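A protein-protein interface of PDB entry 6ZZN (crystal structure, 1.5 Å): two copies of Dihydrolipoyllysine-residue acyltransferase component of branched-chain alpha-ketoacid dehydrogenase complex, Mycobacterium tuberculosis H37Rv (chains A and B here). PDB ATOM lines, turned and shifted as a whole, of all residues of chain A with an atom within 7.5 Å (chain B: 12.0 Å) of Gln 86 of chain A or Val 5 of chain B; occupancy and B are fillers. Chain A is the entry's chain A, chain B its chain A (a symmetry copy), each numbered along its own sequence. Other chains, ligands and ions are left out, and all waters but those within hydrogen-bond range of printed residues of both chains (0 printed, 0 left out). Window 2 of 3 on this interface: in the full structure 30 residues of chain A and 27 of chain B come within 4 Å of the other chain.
No position is printed for both chains.
Of the 10 printed residues of chain A, 7 touch a printed residue of chain B.
Among the printed residues, no Asp or Glu carboxylate lies within 4 Å of a Lys or Arg side-chain nitrogen of the other chain.
The backbone NH of Val 8 of chain B sits at hydrogen-bond distance from the backbone carbonyl oxygen of Pro 85 of chain A (2.9 Å).
The backbone carbonyl oxygen (O) of Val 87 of chain A sits at hydrogen-bond distance from the backbone NH (N) of Arg 6 of chain B (2.8 Å).
The backbone NH (N) of Val 89 of chain A is in hydrogen-bond range of the backbone carbonyl oxygen (O) of Asp 4 of chain B, at 2.8 Å.
CZ3 of Trp 78 of chain A touches CG2 of Val 8 of chain B (3.8 Å).
CH2 of Trp 78 of chain A touches CB of Ala 16 of chain B, at 3.5 Å.
Gln 86 of chain A touches Val 5 of chain B (OE1 to CG1, 3.5 Å).
Arg 6 of chain B touches Gln 86 of chain A.
Gln 86 of chain A touches Val 8 of chain B (CA to CG2, 3.8 Å).
Val 87 of chain A touches Val 5 of chain B.
Val 8 of chain B touches Val 87 of chain A (CG2 to CG2, 3.95 Å).
Asp 4 of chain B touches His 88 of chain A.
CG2 of Val 5 of chain B touches NE2 of His 88 of chain A (3.7 Å).
NE2 of His 12 of chain B touches O of Val 204 of chain A, 3.7 Å away.
The backbone carbonyl oxygen (O) of Thr 77 of chain A sits at hydrogen-bond distance from the backbone NH (N) of His 88 of chain A, 2.9 Å away.
NE1 of Trp 78 of chain A is in hydrogen-bond range of OD1 of Asp 80 of chain A (3.0 Å).
The backbone NH (N) of Val 79 of chain A lies within hydrogen-bond range of the backbone carbonyl oxygen (O) of Gln 86 of chain A.
A ring nitrogen (NE2) of His 88 of chain A sits at hydrogen-bond distance from the side-chain amide oxygen (OE1) of Gln 86 of chain A (2.8 Å).
The side-chain carboxylate (OD2) of Asp 4 of chain B is in salt-bridge range of the guanidinium group (NH2) of Arg 6 of chain B (2.9 Å).
The side-chain hydroxyl of Thr 20 of chain B is in hydrogen-bond range of the backbone carbonyl oxygen of Ala 16 of chain B, at 3.0 Å.
Of the printed residues of chain B, Gln 86 of chain A touches Val 5, Arg 6 and Val 8.
Of chain A, only Gln 86, Val 87 and His 88 come within 4 Å of Val 5 of chain B.
No residue of chain B comes within 4 Å of Val 79 of chain A.
No residue of chain B comes within 4 Å of Asp 80 of chain A.
Of chain B, only Pro 7 and Val 8 come within 4 Å of Pro 85 of chain A.
Of the printed residues of chain B, Val 87 of chain A touches Asp 4 (3.6 Å), Val 5 (3.7 Å), Arg 6 (2.8 Å) and Val 8 (3.95 Å).
Of the printed residues of chain A, Arg 6 of chain B touches Gln 86 (3.5 Å), Val 87 (2.8 Å) and Val 89 (3.5 Å).
Printed residues of chain A within 4 Å of Val 8 of chain B: Trp 78 (3.8 Å), Pro 85 (2.9 Å), Gln 86 (3.8 Å) and Val 87 (3.95 Å).
Gly 10 of chain B touches none of the printed residues of chain A.
The nearest residue of chain B that does not touch Gln 86 of chain A is Pro 7 of chain B (4.1 Å).
The nearest printed residue of chain A that does not touch Pro 7 of chain B is Gln 86 of chain A (4.1 Å).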
ATOM      1  N   THR A  77      16.295   6.893   5.275  1.00  0.00           N
ATOM      2  CA  THR A  77      16.108   7.358   6.640  1.00  0.00           C
ATOM      3  C   THR A  77      14.909   8.283   6.727  1.00  0.00           C
ATOM      4  O   THR A  77      14.715   9.127   5.851  1.00  0.00           O
ATOM      5  CB  THR A  77      17.373   8.135   7.072  1.00  0.00           C
ATOM      6  OG1 THR A  77      18.479   7.227   7.134  1.00  0.00           O
ATOM      7  CG2 THR A  77      17.212   8.836   8.402  1.00  0.00           C
ATOM      8  N   TRP A  78      14.127   8.146   7.806  1.00  0.00           N
ATOM      9  CA  TRP A  78      13.036   9.073   8.087  1.00  0.00           C
ATOM     10  C   TRP A  78      13.654  10.325   8.734  1.00  0.00           C
ATOM     11  O   TRP A  78      14.375  10.213   9.725  1.00  0.00           O
ATOM     12  CB  TRP A  78      12.071   8.434   9.087  1.00  0.00           C
ATOM     13  CG  TRP A  78      10.988   9.360   9.554  1.00  0.00           C
ATOM     14  CD1 TRP A  78      10.996  10.135  10.679  1.00  0.00           C
ATOM     15  CD2 TRP A  78       9.724   9.585   8.920  1.00  0.00           C
ATOM     16  NE1 TRP A  78       9.813  10.831  10.781  1.00  0.00           N
ATOM     17  CE2 TRP A  78       9.011  10.502   9.718  1.00  0.00           C
ATOM     18  CE3 TRP A  78       9.122   9.092   7.758  1.00  0.00           C
ATOM     19  CZ2 TRP A  78       7.723  10.923   9.397  1.00  0.00           C
ATOM     20  CZ3 TRP A  78       7.849   9.518   7.438  1.00  0.00           C
ATOM     21  CH2 TRP A  78       7.169  10.430   8.247  1.00  0.00           C
ATOM     22  N   VAL A  79      13.355  11.490   8.193  1.00  0.00           N
ATOM     23  CA  VAL A  79      13.882  12.746   8.723  1.00  0.00           C
ATOM     24  C   VAL A  79      12.735  13.648   9.169  1.00  0.00           C
ATOM     25  O   VAL A  79      11.840  13.941   8.379  1.00  0.00           O
ATOM     26  CB  VAL A  79      14.793  13.437   7.686  1.00  0.00           C
ATOM     27  CG1 VAL A  79      15.230  14.819   8.171  1.00  0.00           C
ATOM     28  CG2 VAL A  79      16.000  12.565   7.360  1.00  0.00           C
ATOM     29  N   ASP A  80      12.735  14.037  10.448  1.00  0.00           N
ATOM     30  CA  ASP A  80      11.699  14.907  11.002  1.00  0.00           C
ATOM     31  C   ASP A  80      12.042  16.353  10.687  1.00  0.00           C
ATOM     32  O   ASP A  80      13.026  16.870  11.223  1.00  0.00           O
ATOM     33  CB  ASP A  80      11.599  14.719  12.527  1.00  0.00           C
ATOM     34  CG  ASP A  80      11.069  13.363  12.961  1.00  0.00           C
ATOM     35  OD1 ASP A  80       9.857  13.110  12.770  1.00  0.00           O
ATOM     36  OD2 ASP A  80      11.865  12.562  13.512  1.00  0.00           O
ATOM     37  N   PRO A  85       8.248  16.422   7.568  1.00  0.00           N
ATOM     38  CA  PRO A  85       8.749  15.036   7.463  1.00  0.00           C
ATOM     39  C   PRO A  85       9.196  14.703   6.049  1.00  0.00           C
ATOM     40  O   PRO A  85       8.539  15.063   5.070  1.00  0.00           O
ATOM     41  CB  PRO A  85       7.547  14.186   7.872  1.00  0.00           C
ATOM     42  CG  PRO A  85       6.352  15.068   7.596  1.00  0.00           C
ATOM     43  CD  PRO A  85       6.804  16.461   7.872  1.00  0.00           C
ATOM     44  N   GLN A  86      10.315  13.976   5.937  1.00  0.00           N
ATOM     45  CA  GLN A  86      10.879  13.627   4.640  1.00  0.00           C
ATOM     46  C   GLN A  86      11.511  12.249   4.715  1.00  0.00           C
ATOM     47  O   GLN A  86      11.915  11.821   5.789  1.00  0.00           O
ATOM     48  CB  GLN A  86      12.014  14.607   4.294  1.00  0.00           C
ATOM     49  CG  GLN A  86      11.593  16.075   4.269  1.00  0.00           C
ATOM     50  CD  GLN A  86      12.769  16.992   4.071  1.00  0.00           C
ATOM     51  OE1 GLN A  86      13.909  16.680   4.440  1.00  0.00           O
ATOM     52  NE2 GLN A  86      12.513  18.160   3.483  1.00  0.00           N
ATOM     53  N   VAL A  87      11.658  11.597   3.569  1.00  0.00           N
ATOM     54  CA  VAL A  87      12.406  10.354   3.494  1.00  0.00           C
ATOM     55  C   VAL A  87      13.673  10.703   2.711  1.00  0.00           C
ATOM     56  O   VAL A  87      13.583  11.280   1.626  1.00  0.00           O
ATOM     57  CB  VAL A  87      11.626   9.215   2.810  1.00  0.00           C
ATOM     58  CG1 VAL A  87      12.545   8.026   2.539  1.00  0.00           C
ATOM     59  CG2 VAL A  87      10.430   8.790   3.663  1.00  0.00           C
ATOM     60  N   HIS A  88      14.840  10.410   3.273  1.00  0.00           N
ATOM     61  CA  HIS A  88      16.102  10.647   2.594  1.00  0.00           C
ATOM     62  C   HIS A  88      16.593   9.305   2.090  1.00  0.00           C
ATOM     63  O   HIS A  88      16.918   8.415   2.879  1.00  0.00           O
ATOM     64  CB  HIS A  88      17.110  11.270   3.564  1.00  0.00           C
ATOM     65  CG  HIS A  88      16.778  12.690   3.918  1.00  0.00           C
ATOM     66  ND1 HIS A  88      17.769  13.592   4.266  1.00  0.00           N
ATOM     67  CD2 HIS A  88      15.576  13.322   3.948  1.00  0.00           C
ATOM     68  CE1 HIS A  88      17.144  14.738   4.510  1.00  0.00           C
ATOM     69  NE2 HIS A  88      15.823  14.626   4.338  1.00  0.00           N
ATOM     70  N   VAL A  89      16.607   9.151   0.774  1.00  0.00           N
ATOM     71  CA  VAL A  89      17.018   7.904   0.138  1.00  0.00           C
ATOM     72  C   VAL A  89      18.501   7.996  -0.147  1.00  0.00           C
ATOM     73  O   VAL A  89      18.944   8.942  -0.800  1.00  0.00           O
ATOM     74  CB  VAL A  89      16.196   7.679  -1.140  1.00  0.00           C
ATOM     75  CG1 VAL A  89      16.674   6.445  -1.892  1.00  0.00           C
ATOM     76  CG2 VAL A  89      14.712   7.557  -0.800  1.00  0.00           C
ATOM     77  N   VAL A 204       8.357   4.742   6.552  1.00  0.00           N
ATOM     78  CA  VAL A 204       9.159   4.893   5.346  1.00  0.00           C
ATOM     79  C   VAL A 204       8.800   3.921   4.250  1.00  0.00           C
ATOM     80  O   VAL A 204       8.659   4.323   3.088  1.00  0.00           O
ATOM     81  CB  VAL A 204      10.663   4.745   5.723  1.00  0.00           C
ATOM     82  CG1 VAL A 204      11.553   4.835   4.489  1.00  0.00           C
ATOM     83  CG2 VAL A 204      11.064   5.779   6.758  1.00  0.00           C
ATOM     84  N   ASP B   4      18.800  12.593  -2.249  1.00  0.00           N
ATOM     85  CA  ASP B   4      17.471  12.223  -2.747  1.00  0.00           C
ATOM     86  C   ASP B   4      16.478  12.388  -1.606  1.00  0.00           C
ATOM     87  O   ASP B   4      16.213  11.463  -0.840  1.00  0.00           O
ATOM     88  CB  ASP B   4      17.483  10.791  -3.301  1.00  0.00           C
ATOM     89  CG  ASP B   4      16.223  10.358  -4.032  1.00  0.00           C
ATOM     90  OD1 ASP B   4      15.238  11.133  -4.033  1.00  0.00           O
ATOM     91  OD2 ASP B   4      16.216   9.234  -4.587  1.00  0.00           O
ATOM     92  N   VAL B   5      15.961  13.598  -1.473  1.00  0.00           N
ATOM     93  CA  VAL B   5      15.031  13.955  -0.420  1.00  0.00           C
ATOM     94  C   VAL B   5      13.605  13.921  -0.945  1.00  0.00           C
ATOM     95  O   VAL B   5      13.276  14.580  -1.940  1.00  0.00           O
ATOM     96  CB  VAL B   5      15.403  15.350   0.133  1.00  0.00           C
ATOM     97  CG1 VAL B   5      14.339  15.862   1.090  1.00  0.00           C
ATOM     98  CG2 VAL B   5      16.768  15.308   0.808  1.00  0.00           C
ATOM     99  N   ARG B   6      12.741  13.190  -0.252  1.00  0.00           N
ATOM    100  CA  ARG B   6      11.355  13.043  -0.655  1.00  0.00           C
ATOM    101  C   ARG B   6      10.418  13.496   0.436  1.00  0.00           C
ATOM    102  O   ARG B   6      10.138  12.748   1.365  1.00  0.00           O
ATOM    103  CB  ARG B   6      11.082  11.574  -0.997  1.00  0.00           C
ATOM    104  CG  ARG B   6      11.965  11.090  -2.124  1.00  0.00           C
ATOM    105  CD  ARG B   6      11.892   9.602  -2.285  1.00  0.00           C
ATOM    106  NE  ARG B   6      12.868   9.145  -3.271  1.00  0.00           N
ATOM    107  CZ  ARG B   6      12.836   7.956  -3.861  1.00  0.00           C
ATOM    108  NH1 ARG B   6      11.867   7.095  -3.582  1.00  0.00           N
ATOM    109  NH2 ARG B   6      13.770   7.621  -4.739  1.00  0.00           N
ATOM    110  N   PRO B   7       9.874  14.715   0.323  1.00  0.00           N
ATOM    111  CA  PRO B   7       8.927  15.191   1.343  1.00  0.00           C
ATOM    112  C   PRO B   7       7.728  14.248   1.473  1.00  0.00           C
ATOM    113  O   PRO B   7       7.271  13.693   0.478  1.00  0.00           O
ATOM    114  CB  PRO B   7       8.521  16.569   0.827  1.00  0.00           C
ATOM    115  CG  PRO B   7       9.676  17.000  -0.056  1.00  0.00           C
ATOM    116  CD  PRO B   7      10.106  15.730  -0.723  1.00  0.00           C
ATOM    117  N   VAL B   8       7.292  13.988   2.703  1.00  0.00           N
ATOM    118  CA  VAL B   8       6.188  13.065   2.950  1.00  0.00           C
ATOM    119  C   VAL B   8       4.853  13.802   2.881  1.00  0.00           C
ATOM    120  O   VAL B   8       4.644  14.746   3.636  1.00  0.00           O
ATOM    121  CB  VAL B   8       6.397  12.349   4.297  1.00  0.00           C
ATOM    122  CG1 VAL B   8       5.251  11.403   4.593  1.00  0.00           C
ATOM    123  CG2 VAL B   8       7.720  11.592   4.302  1.00  0.00           C
ATOM    124  N   HIS B   9       3.972  13.405   1.945  1.00  0.00           N
ATOM    125  CA  HIS B   9       2.679  14.065   1.735  1.00  0.00           C
ATOM    126  C   HIS B   9       1.515  13.069   1.484  1.00  0.00           C
ATOM    127  O   HIS B   9       1.763  11.896   1.209  1.00  0.00           O
ATOM    128  CB  HIS B   9       2.799  15.041   0.551  1.00  0.00           C
ATOM    129  CG  HIS B   9       3.675  16.221   0.816  1.00  0.00           C
ATOM    130  ND1 HIS B   9       3.364  17.142   1.801  1.00  0.00           N
ATOM    131  CD2 HIS B   9       4.780  16.642   0.156  1.00  0.00           C
ATOM    132  CE1 HIS B   9       4.298  18.081   1.721  1.00  0.00           C
ATOM    133  NE2 HIS B   9       5.176  17.816   0.754  1.00  0.00           N
ATOM    134  N   GLY B  10       0.279  13.569   1.569  1.00  0.00           N
ATOM    135  CA  GLY B  10      -0.961  12.834   1.324  1.00  0.00           C
ATOM    136  C   GLY B  10      -1.028  11.439   1.920  1.00  0.00           C
ATOM    137  O   GLY B  10      -0.836  11.263   3.125  1.00  0.00           O
ATOM    138  N   HIS B  12       1.033   8.905   1.932  1.00  0.00           N
ATOM    139  CA  HIS B  12       2.223   8.497   2.682  1.00  0.00           C
ATOM    140  C   HIS B  12       2.206   9.138   4.077  1.00  0.00           C
ATOM    141  O   HIS B  12       2.477   8.461   5.069  1.00  0.00           O
ATOM    142  CB  HIS B  12       3.494   8.912   1.914  1.00  0.00           C
ATOM    143  CG  HIS B  12       4.760   8.238   2.359  1.00  0.00           C
ATOM    144  ND1 HIS B  12       5.802   8.018   1.475  1.00  0.00           N
ATOM    145  CD2 HIS B  12       5.121   7.770   3.579  1.00  0.00           C
ATOM    146  CE1 HIS B  12       6.754   7.428   2.180  1.00  0.00           C
ATOM    147  NE2 HIS B  12       6.390   7.261   3.450  1.00  0.00           N
ATOM    148  N   ALA B  13       1.876  10.435   4.155  1.00  0.00           N
ATOM    149  CA  ALA B  13       1.839  11.169   5.418  1.00  0.00           C
ATOM    150  C   ALA B  13       0.800  10.600   6.353  1.00  0.00           C
ATOM    151  O   ALA B  13       1.081  10.448   7.546  1.00  0.00           O
ATOM    152  CB  ALA B  13       1.582  12.644   5.170  1.00  0.00           C
ATOM    153  N   ARG B  14      -0.395  10.249   5.813  1.00  0.00           N
ATOM    154  CA  ARG B  14      -1.451   9.626   6.609  1.00  0.00           C
ATOM    155  C   ARG B  14      -0.957   8.304   7.202  1.00  0.00           C
ATOM    156  O   ARG B  14      -1.123   8.080   8.398  1.00  0.00           O
ATOM    157  CB  ARG B  14      -2.723   9.401   5.772  1.00  0.00           C
ATOM    158  N   MET B  15      -0.285   7.461   6.383  1.00  0.00           N
ATOM    159  CA  MET B  15       0.264   6.176   6.833  1.00  0.00           C
ATOM    160  C   MET B  15       1.241   6.392   8.005  1.00  0.00           C
ATOM    161  O   MET B  15       1.058   5.788   9.059  1.00  0.00           O
ATOM    162  CB  MET B  15       0.945   5.407   5.664  1.00  0.00           C
ATOM    163  CG  MET B  15       1.725   4.135   6.103  1.00  0.00           C
ATOM    164  SD  MET B  15       2.482   3.133   4.751  1.00  0.00           S
ATOM    165  CE  MET B  15       3.956   4.143   4.383  1.00  0.00           C
ATOM    166  N   ALA B  16       2.209   7.317   7.855  1.00  0.00           N
ATOM    167  CA  ALA B  16       3.205   7.588   8.901  1.00  0.00           C
ATOM    168  C   ALA B  16       2.619   8.085  10.238  1.00  0.00           C
ATOM    169  O   ALA B  16       3.054   7.642  11.298  1.00  0.00           O
ATOM    170  CB  ALA B  16       4.242   8.572   8.392  1.00  0.00           C
ATOM    171  N   GLU B  17       1.640   8.995  10.192  1.00  0.00           N
ATOM    172  CA  GLU B  17       1.010   9.509  11.408  1.00  0.00           C
ATOM    173  C   GLU B  17       0.290   8.376  12.149  1.00  0.00           C
ATOM    174  O   GLU B  17       0.349   8.299  13.376  1.00  0.00           O
ATOM    175  CB  GLU B  17      -0.004  10.613  11.062  1.00  0.00           C
ATOM    176  N   THR B  20       2.879   5.903  13.775  1.00  0.00           N
ATOM    177  CA  THR B  20       3.486   6.491  14.966  1.00  0.00           C
ATOM    178  C   THR B  20       2.547   6.422  16.173  1.00  0.00           C
ATOM    179  O   THR B  20       2.975   6.094  17.283  1.00  0.00           O
ATOM    180  CB  THR B  20       3.878   7.940  14.660  1.00  0.00           C
ATOM    181  OG1 THR B  20       4.881   7.936  13.635  1.00  0.00           O
ATOM    182  CG2 THR B  20       4.376   8.690  15.890  1.00  0.00           C
